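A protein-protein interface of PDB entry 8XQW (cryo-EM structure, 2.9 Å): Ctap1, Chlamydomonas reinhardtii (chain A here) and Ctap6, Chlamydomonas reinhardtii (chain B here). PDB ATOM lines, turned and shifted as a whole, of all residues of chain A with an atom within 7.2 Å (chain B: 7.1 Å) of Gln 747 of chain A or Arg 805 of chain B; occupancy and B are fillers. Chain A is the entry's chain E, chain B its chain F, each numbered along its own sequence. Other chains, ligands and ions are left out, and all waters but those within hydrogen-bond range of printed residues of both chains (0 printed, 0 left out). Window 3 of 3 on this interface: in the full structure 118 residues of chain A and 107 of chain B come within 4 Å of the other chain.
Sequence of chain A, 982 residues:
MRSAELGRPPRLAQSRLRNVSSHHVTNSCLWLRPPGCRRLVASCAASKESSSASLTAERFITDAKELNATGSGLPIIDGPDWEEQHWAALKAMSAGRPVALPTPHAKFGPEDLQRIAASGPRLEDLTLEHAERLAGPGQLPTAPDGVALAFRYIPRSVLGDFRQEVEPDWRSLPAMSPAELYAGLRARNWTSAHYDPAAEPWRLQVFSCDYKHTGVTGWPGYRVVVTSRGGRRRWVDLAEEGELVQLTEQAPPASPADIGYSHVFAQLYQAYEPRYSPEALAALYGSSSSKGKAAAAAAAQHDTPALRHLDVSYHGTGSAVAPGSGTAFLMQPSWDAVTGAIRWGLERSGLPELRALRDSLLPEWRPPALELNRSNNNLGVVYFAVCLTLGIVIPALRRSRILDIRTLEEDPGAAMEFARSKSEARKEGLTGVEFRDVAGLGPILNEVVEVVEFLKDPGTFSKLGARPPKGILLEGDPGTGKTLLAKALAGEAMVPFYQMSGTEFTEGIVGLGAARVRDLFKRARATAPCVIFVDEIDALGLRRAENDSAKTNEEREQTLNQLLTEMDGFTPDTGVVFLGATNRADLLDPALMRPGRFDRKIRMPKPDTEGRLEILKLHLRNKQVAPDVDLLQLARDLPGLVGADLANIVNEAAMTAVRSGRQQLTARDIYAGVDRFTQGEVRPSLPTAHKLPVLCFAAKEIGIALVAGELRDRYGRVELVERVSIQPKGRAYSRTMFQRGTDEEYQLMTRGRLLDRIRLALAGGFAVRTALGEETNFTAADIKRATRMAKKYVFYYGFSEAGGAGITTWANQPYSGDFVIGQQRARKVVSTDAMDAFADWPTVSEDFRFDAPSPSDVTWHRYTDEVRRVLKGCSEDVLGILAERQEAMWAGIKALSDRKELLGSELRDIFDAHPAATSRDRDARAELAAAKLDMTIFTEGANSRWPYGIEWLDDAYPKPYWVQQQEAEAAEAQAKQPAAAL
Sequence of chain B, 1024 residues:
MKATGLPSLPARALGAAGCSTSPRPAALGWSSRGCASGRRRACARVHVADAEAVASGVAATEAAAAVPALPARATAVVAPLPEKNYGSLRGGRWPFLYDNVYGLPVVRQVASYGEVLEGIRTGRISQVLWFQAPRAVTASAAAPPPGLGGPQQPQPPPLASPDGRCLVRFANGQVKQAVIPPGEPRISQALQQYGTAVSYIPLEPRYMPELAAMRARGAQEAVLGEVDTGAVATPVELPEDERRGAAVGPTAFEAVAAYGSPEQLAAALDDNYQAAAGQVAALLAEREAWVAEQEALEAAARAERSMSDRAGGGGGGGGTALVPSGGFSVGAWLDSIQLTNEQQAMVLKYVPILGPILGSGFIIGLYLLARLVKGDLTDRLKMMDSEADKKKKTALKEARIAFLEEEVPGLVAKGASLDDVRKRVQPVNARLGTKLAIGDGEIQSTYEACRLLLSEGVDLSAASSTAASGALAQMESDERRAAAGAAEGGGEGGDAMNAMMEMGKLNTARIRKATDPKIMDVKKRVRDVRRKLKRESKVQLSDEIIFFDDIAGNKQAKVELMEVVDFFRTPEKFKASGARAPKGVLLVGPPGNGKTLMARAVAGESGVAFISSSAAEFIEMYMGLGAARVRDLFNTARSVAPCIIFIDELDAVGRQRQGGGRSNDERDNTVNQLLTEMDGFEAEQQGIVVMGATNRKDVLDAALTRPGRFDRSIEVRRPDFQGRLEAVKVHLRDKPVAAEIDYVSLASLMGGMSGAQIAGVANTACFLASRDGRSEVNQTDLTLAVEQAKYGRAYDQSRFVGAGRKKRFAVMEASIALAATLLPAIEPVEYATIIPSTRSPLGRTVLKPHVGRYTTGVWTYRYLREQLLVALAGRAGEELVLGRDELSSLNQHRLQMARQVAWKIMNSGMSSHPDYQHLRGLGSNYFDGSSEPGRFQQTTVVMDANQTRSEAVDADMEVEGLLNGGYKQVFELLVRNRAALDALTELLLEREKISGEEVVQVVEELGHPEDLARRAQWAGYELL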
ATOM      1  N   THR A 742      18.584  11.558 -22.719  1.00  0.00           N
ATOM      2  CA  THR A 742      19.409  11.812 -23.885  1.00  0.00           C
ATOM      3  C   THR A 742      19.134  10.774 -24.967  1.00  0.00           C
ATOM      4  O   THR A 742      18.609   9.689 -24.708  1.00  0.00           O
ATOM      5  CB  THR A 742      20.885  11.795 -23.509  1.00  0.00           C
ATOM      6  OG1 THR A 742      21.670  11.630 -24.694  1.00  0.00           O
ATOM      7  CG2 THR A 742      21.167  10.660 -22.545  1.00  0.00           C
ATOM      8  N   ASP A 743      19.504  11.120 -26.200  1.00  0.00           N
ATOM      9  CA  ASP A 743      19.245  10.227 -27.323  1.00  0.00           C
ATOM     10  C   ASP A 743      19.930   8.881 -27.149  1.00  0.00           C
ATOM     11  O   ASP A 743      19.445   7.870 -27.665  1.00  0.00           O
ATOM     12  CB  ASP A 743      19.687  10.879 -28.628  1.00  0.00           C
ATOM     13  CG  ASP A 743      19.318  10.055 -29.844  1.00  0.00           C
ATOM     14  OD1 ASP A 743      19.967   9.016 -30.087  1.00  0.00           O
ATOM     15  OD2 ASP A 743      18.371  10.442 -30.558  1.00  0.00           O
ATOM     16  N   GLU A 744      21.053   8.842 -26.431  1.00  0.00           N
ATOM     17  CA  GLU A 744      21.697   7.568 -26.142  1.00  0.00           C
ATOM     18  C   GLU A 744      20.736   6.598 -25.475  1.00  0.00           C
ATOM     19  O   GLU A 744      20.857   5.382 -25.648  1.00  0.00           O
ATOM     20  CB  GLU A 744      22.925   7.794 -25.262  1.00  0.00           C
ATOM     21  CG  GLU A 744      23.519   6.531 -24.664  1.00  0.00           C
ATOM     22  CD  GLU A 744      24.178   5.644 -25.705  1.00  0.00           C
ATOM     23  OE1 GLU A 744      24.373   4.444 -25.424  1.00  0.00           O
ATOM     24  OE2 GLU A 744      24.506   6.146 -26.799  1.00  0.00           O
ATOM     25  N   GLU A 745      19.761   7.115 -24.729  1.00  0.00           N
ATOM     26  CA  GLU A 745      18.805   6.244 -24.065  1.00  0.00           C
ATOM     27  C   GLU A 745      17.880   5.557 -25.055  1.00  0.00           C
ATOM     28  O   GLU A 745      17.437   4.432 -24.803  1.00  0.00           O
ATOM     29  CB  GLU A 745      17.982   7.045 -23.063  1.00  0.00           C
ATOM     30  CG  GLU A 745      18.714   7.388 -21.787  1.00  0.00           C
ATOM     31  CD  GLU A 745      18.651   6.272 -20.775  1.00  0.00           C
ATOM     32  OE1 GLU A 745      17.887   5.313 -21.001  1.00  0.00           O
ATOM     33  OE2 GLU A 745      19.358   6.354 -19.750  1.00  0.00           O
ATOM     34  N   TYR A 746      17.575   6.203 -26.175  1.00  0.00           N
ATOM     35  CA  TYR A 746      16.499   5.758 -27.049  1.00  0.00           C
ATOM     36  C   TYR A 746      16.993   5.089 -28.318  1.00  0.00           C
ATOM     37  O   TYR A 746      16.242   5.009 -29.292  1.00  0.00           O
ATOM     38  CB  TYR A 746      15.594   6.934 -27.401  1.00  0.00           C
ATOM     39  CG  TYR A 746      14.949   7.554 -26.194  1.00  0.00           C
ATOM     40  CD1 TYR A 746      13.727   7.105 -25.737  1.00  0.00           C
ATOM     41  CD2 TYR A 746      15.569   8.574 -25.502  1.00  0.00           C
ATOM     42  CE1 TYR A 746      13.139   7.659 -24.630  1.00  0.00           C
ATOM     43  CE2 TYR A 746      14.988   9.133 -24.396  1.00  0.00           C
ATOM     44  CZ  TYR A 746      13.773   8.673 -23.963  1.00  0.00           C
ATOM     45  OH  TYR A 746      13.185   9.231 -22.855  1.00  0.00           O
ATOM     46  N   GLN A 747      18.232   4.610 -28.342  1.00  0.00           N
ATOM     47  CA  GLN A 747      18.679   3.856 -29.502  1.00  0.00           C
ATOM     48  C   GLN A 747      18.359   2.382 -29.375  1.00  0.00           C
ATOM     49  O   GLN A 747      18.221   1.697 -30.389  1.00  0.00           O
ATOM     50  CB  GLN A 747      20.178   4.039 -29.710  1.00  0.00           C
ATOM     51  CG  GLN A 747      20.616   5.479 -29.761  1.00  0.00           C
ATOM     52  CD  GLN A 747      20.362   6.111 -31.103  1.00  0.00           C
ATOM     53  OE1 GLN A 747      19.626   5.575 -31.929  1.00  0.00           O
ATOM     54  NE2 GLN A 747      20.975   7.260 -31.336  1.00  0.00           N
ATOM     55  N   LEU A 748      18.244   1.882 -28.159  1.00  0.00           N
ATOM     56  CA  LEU A 748      17.999   0.481 -27.899  1.00  0.00           C
ATOM     57  C   LEU A 748      16.633   0.315 -27.258  1.00  0.00           C
ATOM     58  O   LEU A 748      16.008   1.271 -26.805  1.00  0.00           O
ATOM     59  CB  LEU A 748      19.083  -0.092 -26.995  1.00  0.00           C
ATOM     60  CG  LEU A 748      19.970  -1.132 -27.644  1.00  0.00           C
ATOM     61  CD1 LEU A 748      20.650  -0.519 -28.828  1.00  0.00           C
ATOM     62  CD2 LEU A 748      20.979  -1.582 -26.639  1.00  0.00           C
ATOM     63  N   MET A 749      16.172  -0.924 -27.226  1.00  0.00           N
ATOM     64  CA  MET A 749      14.979  -1.264 -26.475  1.00  0.00           C
ATOM     65  C   MET A 749      15.240  -2.603 -25.826  1.00  0.00           C
ATOM     66  O   MET A 749      15.132  -3.634 -26.486  1.00  0.00           O
ATOM     67  CB  MET A 749      13.751  -1.329 -27.371  1.00  0.00           C
ATOM     68  CG  MET A 749      12.532  -1.907 -26.691  1.00  0.00           C
ATOM     69  SD  MET A 749      11.668  -0.709 -25.671  1.00  0.00           S
ATOM     70  CE  MET A 749      10.929   0.319 -26.925  1.00  0.00           C
ATOM     71  N   MET A 835       9.174   8.050 -30.295  1.00  0.00           N
ATOM     72  CA  MET A 835      10.564   8.068 -29.879  1.00  0.00           C
ATOM     73  C   MET A 835      11.110   6.672 -29.645  1.00  0.00           C
ATOM     74  O   MET A 835      12.301   6.441 -29.871  1.00  0.00           O
ATOM     75  CB  MET A 835      10.720   8.897 -28.609  1.00  0.00           C
ATOM     76  CG  MET A 835      12.134   9.335 -28.333  1.00  0.00           C
ATOM     77  SD  MET A 835      12.180  10.558 -27.019  1.00  0.00           S
ATOM     78  CE  MET A 835      10.803  11.585 -27.506  1.00  0.00           C
ATOM     79  N   PHE A 838      12.571   4.390 -32.611  1.00  0.00           N
ATOM     80  CA  PHE A 838      13.928   4.560 -33.104  1.00  0.00           C
ATOM     81  C   PHE A 838      14.716   3.273 -33.096  1.00  0.00           C
ATOM     82  O   PHE A 838      15.875   3.279 -33.515  1.00  0.00           O
ATOM     83  CB  PHE A 838      14.668   5.593 -32.266  1.00  0.00           C
ATOM     84  CG  PHE A 838      14.313   7.001 -32.597  1.00  0.00           C
ATOM     85  CD1 PHE A 838      13.446   7.284 -33.632  1.00  0.00           C
ATOM     86  CD2 PHE A 838      14.846   8.047 -31.872  1.00  0.00           C
ATOM     87  CE1 PHE A 838      13.120   8.585 -33.938  1.00  0.00           C
ATOM     88  CE2 PHE A 838      14.524   9.347 -32.173  1.00  0.00           C
ATOM     89  CZ  PHE A 838      13.660   9.617 -33.208  1.00  0.00           C
ATOM     90  N   ALA A 839      14.132   2.174 -32.635  1.00  0.00           N
ATOM     91  CA  ALA A 839      14.868   0.931 -32.477  1.00  0.00           C
ATOM     92  C   ALA A 839      14.420  -0.135 -33.465  1.00  0.00           C
ATOM     93  O   ALA A 839      14.647  -1.320 -33.224  1.00  0.00           O
ATOM     94  CB  ALA A 839      14.724   0.417 -31.048  1.00  0.00           C
ATOM     95  N   ASP A 840      13.815   0.253 -34.583  1.00  0.00           N
ATOM     96  CA  ASP A 840      13.100  -0.712 -35.404  1.00  0.00           C
ATOM     97  C   ASP A 840      13.816  -1.111 -36.684  1.00  0.00           C
ATOM     98  O   ASP A 840      13.855  -2.303 -36.996  1.00  0.00           O
ATOM     99  CB  ASP A 840      11.717  -0.173 -35.750  1.00  0.00           C
ATOM    100  CG  ASP A 840      10.673  -0.632 -34.771  1.00  0.00           C
ATOM    101  OD1 ASP A 840      11.035  -1.371 -33.836  1.00  0.00           O
ATOM    102  OD2 ASP A 840       9.494  -0.260 -34.931  1.00  0.00           O
ATOM    103  N   TRP A 841      14.377  -0.166 -37.428  1.00  0.00           N
ATOM    104  CA  TRP A 841      14.970  -0.451 -38.731  1.00  0.00           C
ATOM    105  C   TRP A 841      13.918  -1.045 -39.657  1.00  0.00           C
ATOM    106  O   TRP A 841      13.915  -2.258 -39.888  1.00  0.00           O
ATOM    107  CB  TRP A 841      16.167  -1.399 -38.630  1.00  0.00           C
ATOM    108  CG  TRP A 841      17.108  -1.073 -37.541  1.00  0.00           C
ATOM    109  CD1 TRP A 841      17.226   0.107 -36.892  1.00  0.00           C
ATOM    110  CD2 TRP A 841      18.083  -1.942 -36.972  1.00  0.00           C
ATOM    111  NE1 TRP A 841      18.203   0.029 -35.943  1.00  0.00           N
ATOM    112  CE2 TRP A 841      18.745  -1.225 -35.974  1.00  0.00           C
ATOM    113  CE3 TRP A 841      18.454  -3.260 -37.209  1.00  0.00           C
ATOM    114  CZ2 TRP A 841      19.760  -1.776 -35.220  1.00  0.00           C
ATOM    115  CZ3 TRP A 841      19.454  -3.805 -36.455  1.00  0.00           C
ATOM    116  CH2 TRP A 841      20.097  -3.068 -35.475  1.00  0.00           C
ATOM    117  N   PHE B 800      28.686   9.684 -31.755  1.00  0.00           N
ATOM    118  CA  PHE B 800      29.142   9.247 -30.445  1.00  0.00           C
ATOM    119  C   PHE B 800      28.407   7.973 -30.054  1.00  0.00           C
ATOM    120  O   PHE B 800      27.248   7.781 -30.433  1.00  0.00           O
ATOM    121  CB  PHE B 800      28.907  10.334 -29.395  1.00  0.00           C
ATOM    122  CG  PHE B 800      28.970   9.832 -27.983  1.00  0.00           C
ATOM    123  CD1 PHE B 800      30.187   9.546 -27.394  1.00  0.00           C
ATOM    124  CD2 PHE B 800      27.812   9.640 -27.251  1.00  0.00           C
ATOM    125  CE1 PHE B 800      30.250   9.082 -26.096  1.00  0.00           C
ATOM    126  CE2 PHE B 800      27.869   9.176 -25.952  1.00  0.00           C
ATOM    127  CZ  PHE B 800      29.089   8.898 -25.374  1.00  0.00           C
ATOM    128  N   VAL B 801      29.084   7.105 -29.309  1.00  0.00           N
ATOM    129  CA  VAL B 801      28.481   5.899 -28.757  1.00  0.00           C
ATOM    130  C   VAL B 801      28.881   5.798 -27.292  1.00  0.00           C
ATOM    131  O   VAL B 801      30.055   5.983 -26.946  1.00  0.00           O
ATOM    132  CB  VAL B 801      28.882   4.640 -29.545  1.00  0.00           C
ATOM    133  CG1 VAL B 801      28.517   4.795 -31.005  1.00  0.00           C
ATOM    134  CG2 VAL B 801      30.370   4.370 -29.426  1.00  0.00           C
ATOM    135  N   GLY B 802      27.902   5.547 -26.430  1.00  0.00           N
ATOM    136  CA  GLY B 802      28.183   5.435 -25.017  1.00  0.00           C
ATOM    137  C   GLY B 802      29.017   4.213 -24.697  1.00  0.00           C
ATOM    138  O   GLY B 802      29.094   3.256 -25.464  1.00  0.00           O
ATOM    139  N   ALA B 803      29.668   4.253 -23.537  1.00  0.00           N
ATOM    140  CA  ALA B 803      30.450   3.100 -23.114  1.00  0.00           C
ATOM    141  C   ALA B 803      29.567   1.952 -22.654  1.00  0.00           C
ATOM    142  O   ALA B 803      30.060   0.835 -22.472  1.00  0.00           O
ATOM    143  CB  ALA B 803      31.418   3.493 -22.003  1.00  0.00           C
ATOM    144  N   GLY B 804      28.279   2.201 -22.454  1.00  0.00           N
ATOM    145  CA  GLY B 804      27.370   1.145 -22.073  1.00  0.00           C
ATOM    146  C   GLY B 804      26.869   0.387 -23.280  1.00  0.00           C
ATOM    147  O   GLY B 804      26.723  -0.836 -23.235  1.00  0.00           O
ATOM    148  N   ARG B 805      26.597   1.107 -24.365  1.00  0.00           N
ATOM    149  CA  ARG B 805      26.213   0.443 -25.601  1.00  0.00           C
ATOM    150  C   ARG B 805      27.392  -0.227 -26.280  1.00  0.00           C
ATOM    151  O   ARG B 805      27.207  -1.268 -26.912  1.00  0.00           O
ATOM    152  CB  ARG B 805      25.561   1.437 -26.559  1.00  0.00           C
ATOM    153  CG  ARG B 805      25.038   0.789 -27.815  1.00  0.00           C
ATOM    154  CD  ARG B 805      24.126   1.702 -28.599  1.00  0.00           C
ATOM    155  NE  ARG B 805      24.610   3.072 -28.629  1.00  0.00           N
ATOM    156  CZ  ARG B 805      24.432   3.894 -29.654  1.00  0.00           C
ATOM    157  NH1 ARG B 805      23.794   3.475 -30.735  1.00  0.00           N
ATOM    158  NH2 ARG B 805      24.899   5.132 -29.604  1.00  0.00           N
ATOM    159  N   LYS B 806      28.594   0.320 -26.140  1.00  0.00           N
ATOM    160  CA  LYS B 806      29.778  -0.262 -26.747  1.00  0.00           C
ATOM    161  C   LYS B 806      30.050  -1.684 -26.285  1.00  0.00           C
ATOM    162  O   LYS B 806      30.512  -2.506 -27.088  1.00  0.00           O
ATOM    163  CB  LYS B 806      30.994   0.609 -26.442  1.00  0.00           C
ATOM    164  CG  LYS B 806      32.160   0.366 -27.359  1.00  0.00           C
ATOM    165  CD  LYS B 806      33.432   0.998 -26.810  1.00  0.00           C
ATOM    166  CE  LYS B 806      33.494   2.486 -27.107  1.00  0.00           C
ATOM    167  NZ  LYS B 806      33.606   2.749 -28.566  1.00  0.00           N
ATOM    168  N   LYS B 807      29.761  -2.009 -25.030  1.00  0.00           N
ATOM    169  CA  LYS B 807      30.018  -3.370 -24.592  1.00  0.00           C
ATOM    170  C   LYS B 807      29.058  -4.363 -25.224  1.00  0.00           C
ATOM    171  O   LYS B 807      29.429  -5.520 -25.428  1.00  0.00           O
ATOM    172  CB  LYS B 807      29.946  -3.483 -23.077  1.00  0.00           C
ATOM    173  CG  LYS B 807      30.728  -4.668 -22.582  1.00  0.00           C
ATOM    174  CD  LYS B 807      30.420  -5.002 -21.151  1.00  0.00           C
ATOM    175  CE  LYS B 807      31.257  -6.181 -20.708  1.00  0.00           C
ATOM    176  NZ  LYS B 807      30.797  -6.737 -19.412  1.00  0.00           N
ATOM    177  N   ARG B 808      27.832  -3.949 -25.539  1.00  0.00           N
ATOM    178  CA  ARG B 808      26.935  -4.830 -26.279  1.00  0.00           C
ATOM    179  C   ARG B 808      27.529  -5.193 -27.629  1.00  0.00           C
ATOM    180  O   ARG B 808      27.570  -6.370 -28.011  1.00  0.00           O
ATOM    181  CB  ARG B 808      25.581  -4.162 -26.468  1.00  0.00           C
ATOM    182  CG  ARG B 808      24.697  -4.209 -25.263  1.00  0.00           C
ATOM    183  CD  ARG B 808      23.263  -4.025 -25.668  1.00  0.00           C
ATOM    184  NE  ARG B 808      22.394  -3.907 -24.508  1.00  0.00           N
ATOM    185  CZ  ARG B 808      21.928  -4.943 -23.826  1.00  0.00           C
ATOM    186  NH1 ARG B 808      22.242  -6.173 -24.193  1.00  0.00           N
ATOM    187  NH2 ARG B 808      21.144  -4.749 -22.779  1.00  0.00           N
ATOM    188  N   PHE B 809      27.963  -4.178 -28.380  1.00  0.00           N
ATOM    189  CA  PHE B 809      28.648  -4.412 -29.641  1.00  0.00           C
ATOM    190  C   PHE B 809      29.786  -5.395 -29.461  1.00  0.00           C
ATOM    191  O   PHE B 809      29.914  -6.359 -30.225  1.00  0.00           O
ATOM    192  CB  PHE B 809      29.196  -3.099 -30.190  1.00  0.00           C
ATOM    193  CG  PHE B 809      28.149  -2.136 -30.644  1.00  0.00           C
ATOM    194  CD1 PHE B 809      26.818  -2.371 -30.420  1.00  0.00           C
ATOM    195  CD2 PHE B 809      28.509  -0.985 -31.304  1.00  0.00           C
ATOM    196  CE1 PHE B 809      25.877  -1.480 -30.841  1.00  0.00           C
ATOM    197  CE2 PHE B 809      27.569  -0.098 -31.728  1.00  0.00           C
ATOM    198  CZ  PHE B 809      26.253  -0.346 -31.498  1.00  0.00           C
ATOM    199  N   ALA B 810      30.631  -5.164 -28.461  1.00  0.00           N
ATOM    200  CA  ALA B 810      31.786  -6.030 -28.288  1.00  0.00           C
ATOM    201  C   ALA B 810      31.369  -7.463 -28.003  1.00  0.00           C
ATOM    202  O   ALA B 810      31.922  -8.399 -28.583  1.00  0.00           O
ATOM    203  CB  ALA B 810      32.680  -5.501 -27.174  1.00  0.00           C
ATOM    204  N   PRO B 836      30.501   1.619 -35.875  1.00  0.00           N
ATOM    205  CA  PRO B 836      29.384   1.692 -36.813  1.00  0.00           C
ATOM    206  C   PRO B 836      29.696   2.613 -37.974  1.00  0.00           C
ATOM    207  O   PRO B 836      30.340   3.650 -37.818  1.00  0.00           O
ATOM    208  CB  PRO B 836      28.241   2.254 -35.961  1.00  0.00           C
ATOM    209  CG  PRO B 836      28.683   2.098 -34.559  1.00  0.00           C
ATOM    210  CD  PRO B 836      30.161   2.213 -34.580  1.00  0.00           C
ATOM    211  N   PRO B 841      24.148   0.257 -38.124  1.00  0.00           N
ATOM    212  CA  PRO B 841      24.266   0.848 -36.789  1.00  0.00           C
ATOM    213  C   PRO B 841      24.807  -0.092 -35.726  1.00  0.00           C
ATOM    214  O   PRO B 841      24.583   0.141 -34.537  1.00  0.00           O
ATOM    215  CB  PRO B 841      22.830   1.267 -36.480  1.00  0.00           C
ATOM    216  CG  PRO B 841      22.008   0.290 -37.212  1.00  0.00           C
ATOM    217  CD  PRO B 841      22.753  -0.067 -38.460  1.00  0.00           C
ATOM    218  N   SER B 889      17.231  -5.059 -28.641  1.00  0.00           N
ATOM    219  CA  SER B 889      16.676  -5.049 -29.978  1.00  0.00           C
ATOM    220  C   SER B 889      17.749  -4.925 -31.041  1.00  0.00           C
ATOM    221  O   SER B 889      17.496  -4.343 -32.095  1.00  0.00           O
ATOM    222  CB  SER B 889      15.682  -3.910 -30.130  1.00  0.00           C
ATOM    223  OG  SER B 889      16.287  -2.839 -30.828  1.00  0.00           O
ATOM    224  N   LEU B 890      18.951  -5.426 -30.776  1.00  0.00           N
ATOM    225  CA  LEU B 890      19.999  -5.434 -31.782  1.00  0.00           C
ATOM    226  C   LEU B 890      19.983  -6.690 -32.633  1.00  0.00           C
ATOM    227  O   LEU B 890      20.602  -6.703 -33.699  1.00  0.00           O
ATOM    228  CB  LEU B 890      21.364  -5.297 -31.116  1.00  0.00           C
ATOM    229  CG  LEU B 890      21.739  -3.931 -30.565  1.00  0.00           C
ATOM    230  CD1 LEU B 890      23.205  -3.922 -30.240  1.00  0.00           C
ATOM    231  CD2 LEU B 890      21.411  -2.849 -31.557  1.00  0.00           C
ATOM    232  N   GLN B 892      17.251  -8.134 -34.145  1.00  0.00           N
ATOM    233  CA  GLN B 892      16.032  -8.341 -34.911  1.00  0.00           C
ATOM    234  C   GLN B 892      16.348  -8.935 -36.278  1.00  0.00           C
ATOM    235  O   GLN B 892      15.717  -9.907 -36.713  1.00  0.00           O
ATOM    236  CB  GLN B 892      15.274  -7.029 -35.046  1.00  0.00           C
ATOM    237  CG  GLN B 892      16.159  -5.830 -35.096  1.00  0.00           C
ATOM    238  CD  GLN B 892      15.387  -4.551 -35.013  1.00  0.00           C
ATOM    239  OE1 GLN B 892      15.789  -3.617 -34.341  1.00  0.00           O
ATOM    240  NE2 GLN B 892      14.274  -4.494 -35.712  1.00  0.00           N
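NE2 of Gln 892 of chain B sits at hydrogen-bond distance from O of Asp 840 of chain A (2.6 Å). O of Ala 839 of chain A sits close to OE1 of Gln 892 of chain B (2.8 Å). O of Met 749 of chain A sits at hydrogen-bond distance from N of Ser 889 of chain B (3.3 Å). The backbone NH of Gly 802 of chain B sits at hydrogen-bond distance from the side-chain carboxylate of Glu 744 of chain A, at 3.5 Å. The backbone carbonyl oxygen (O) of Ala 839 of chain A lies within hydrogen-bond range of the side-chain hydroxyl (OG) of Ser 889 of chain B (3.3 Å). OE2 of Glu 744 of chain A is in salt-bridge range of NH2 of Arg 805 of chain B.
The backbone carbonyl oxygen of Ser 889 of chain B lies close to the side-chain amide oxygen of Gln 892 of chain B (2.9 Å). The backbone NH of Glu 744 of chain A sits close to the side-chain hydroxyl of Thr 742 of chain A (3.3 Å).
CB of Gln 747 of chain A touches NH1 of Arg 805 of chain B, 3.8 Å away. Arg 808 of chain B touches Leu 748 of chain A (NE to CD2, 3.5 Å). CD2 of Leu 890 of chain B touches CD1 of Leu 748 of chain A, 3.7 Å away. Trp 841 of chain A touches Pro 841 of chain B (CZ2 to CG, 3.6 Å). Trp 841 of chain A touches Gln 892 of chain B (CD2 to OE1, 3.9 Å).
Printed residues of chain B within 4 Å of Gln 747 of chain A: Arg 805. No residue of chain A comes within 4 Å of Gly 804 of chain B. Of the printed residues of chain B, Glu 744 of chain A touches Gly 802 and Arg 805. Printed residues of chain B within 4 Å of Trp 841 of chain A: Pro 841 (3.6 Å) and Gln 892 (3.9 Å). Of the printed residues of chain A, Arg 808 of chain B touches Leu 748 (3.5 Å). Ala 810 of chain B touches none of the printed residues of chain A. Thr 742 of chain A touches none of the printed residues of chain B.
Hydrophobic or aromatic side chains of chain B that line the printed part of chain A: Pro 841 and Leu 890. Among the printed residues, Asp or Glu carboxylates within 4 Å of a Lys or Arg side-chain nitrogen of the other chain: Glu 744 of chain A with Arg 805 of chain B (3.0 Å).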
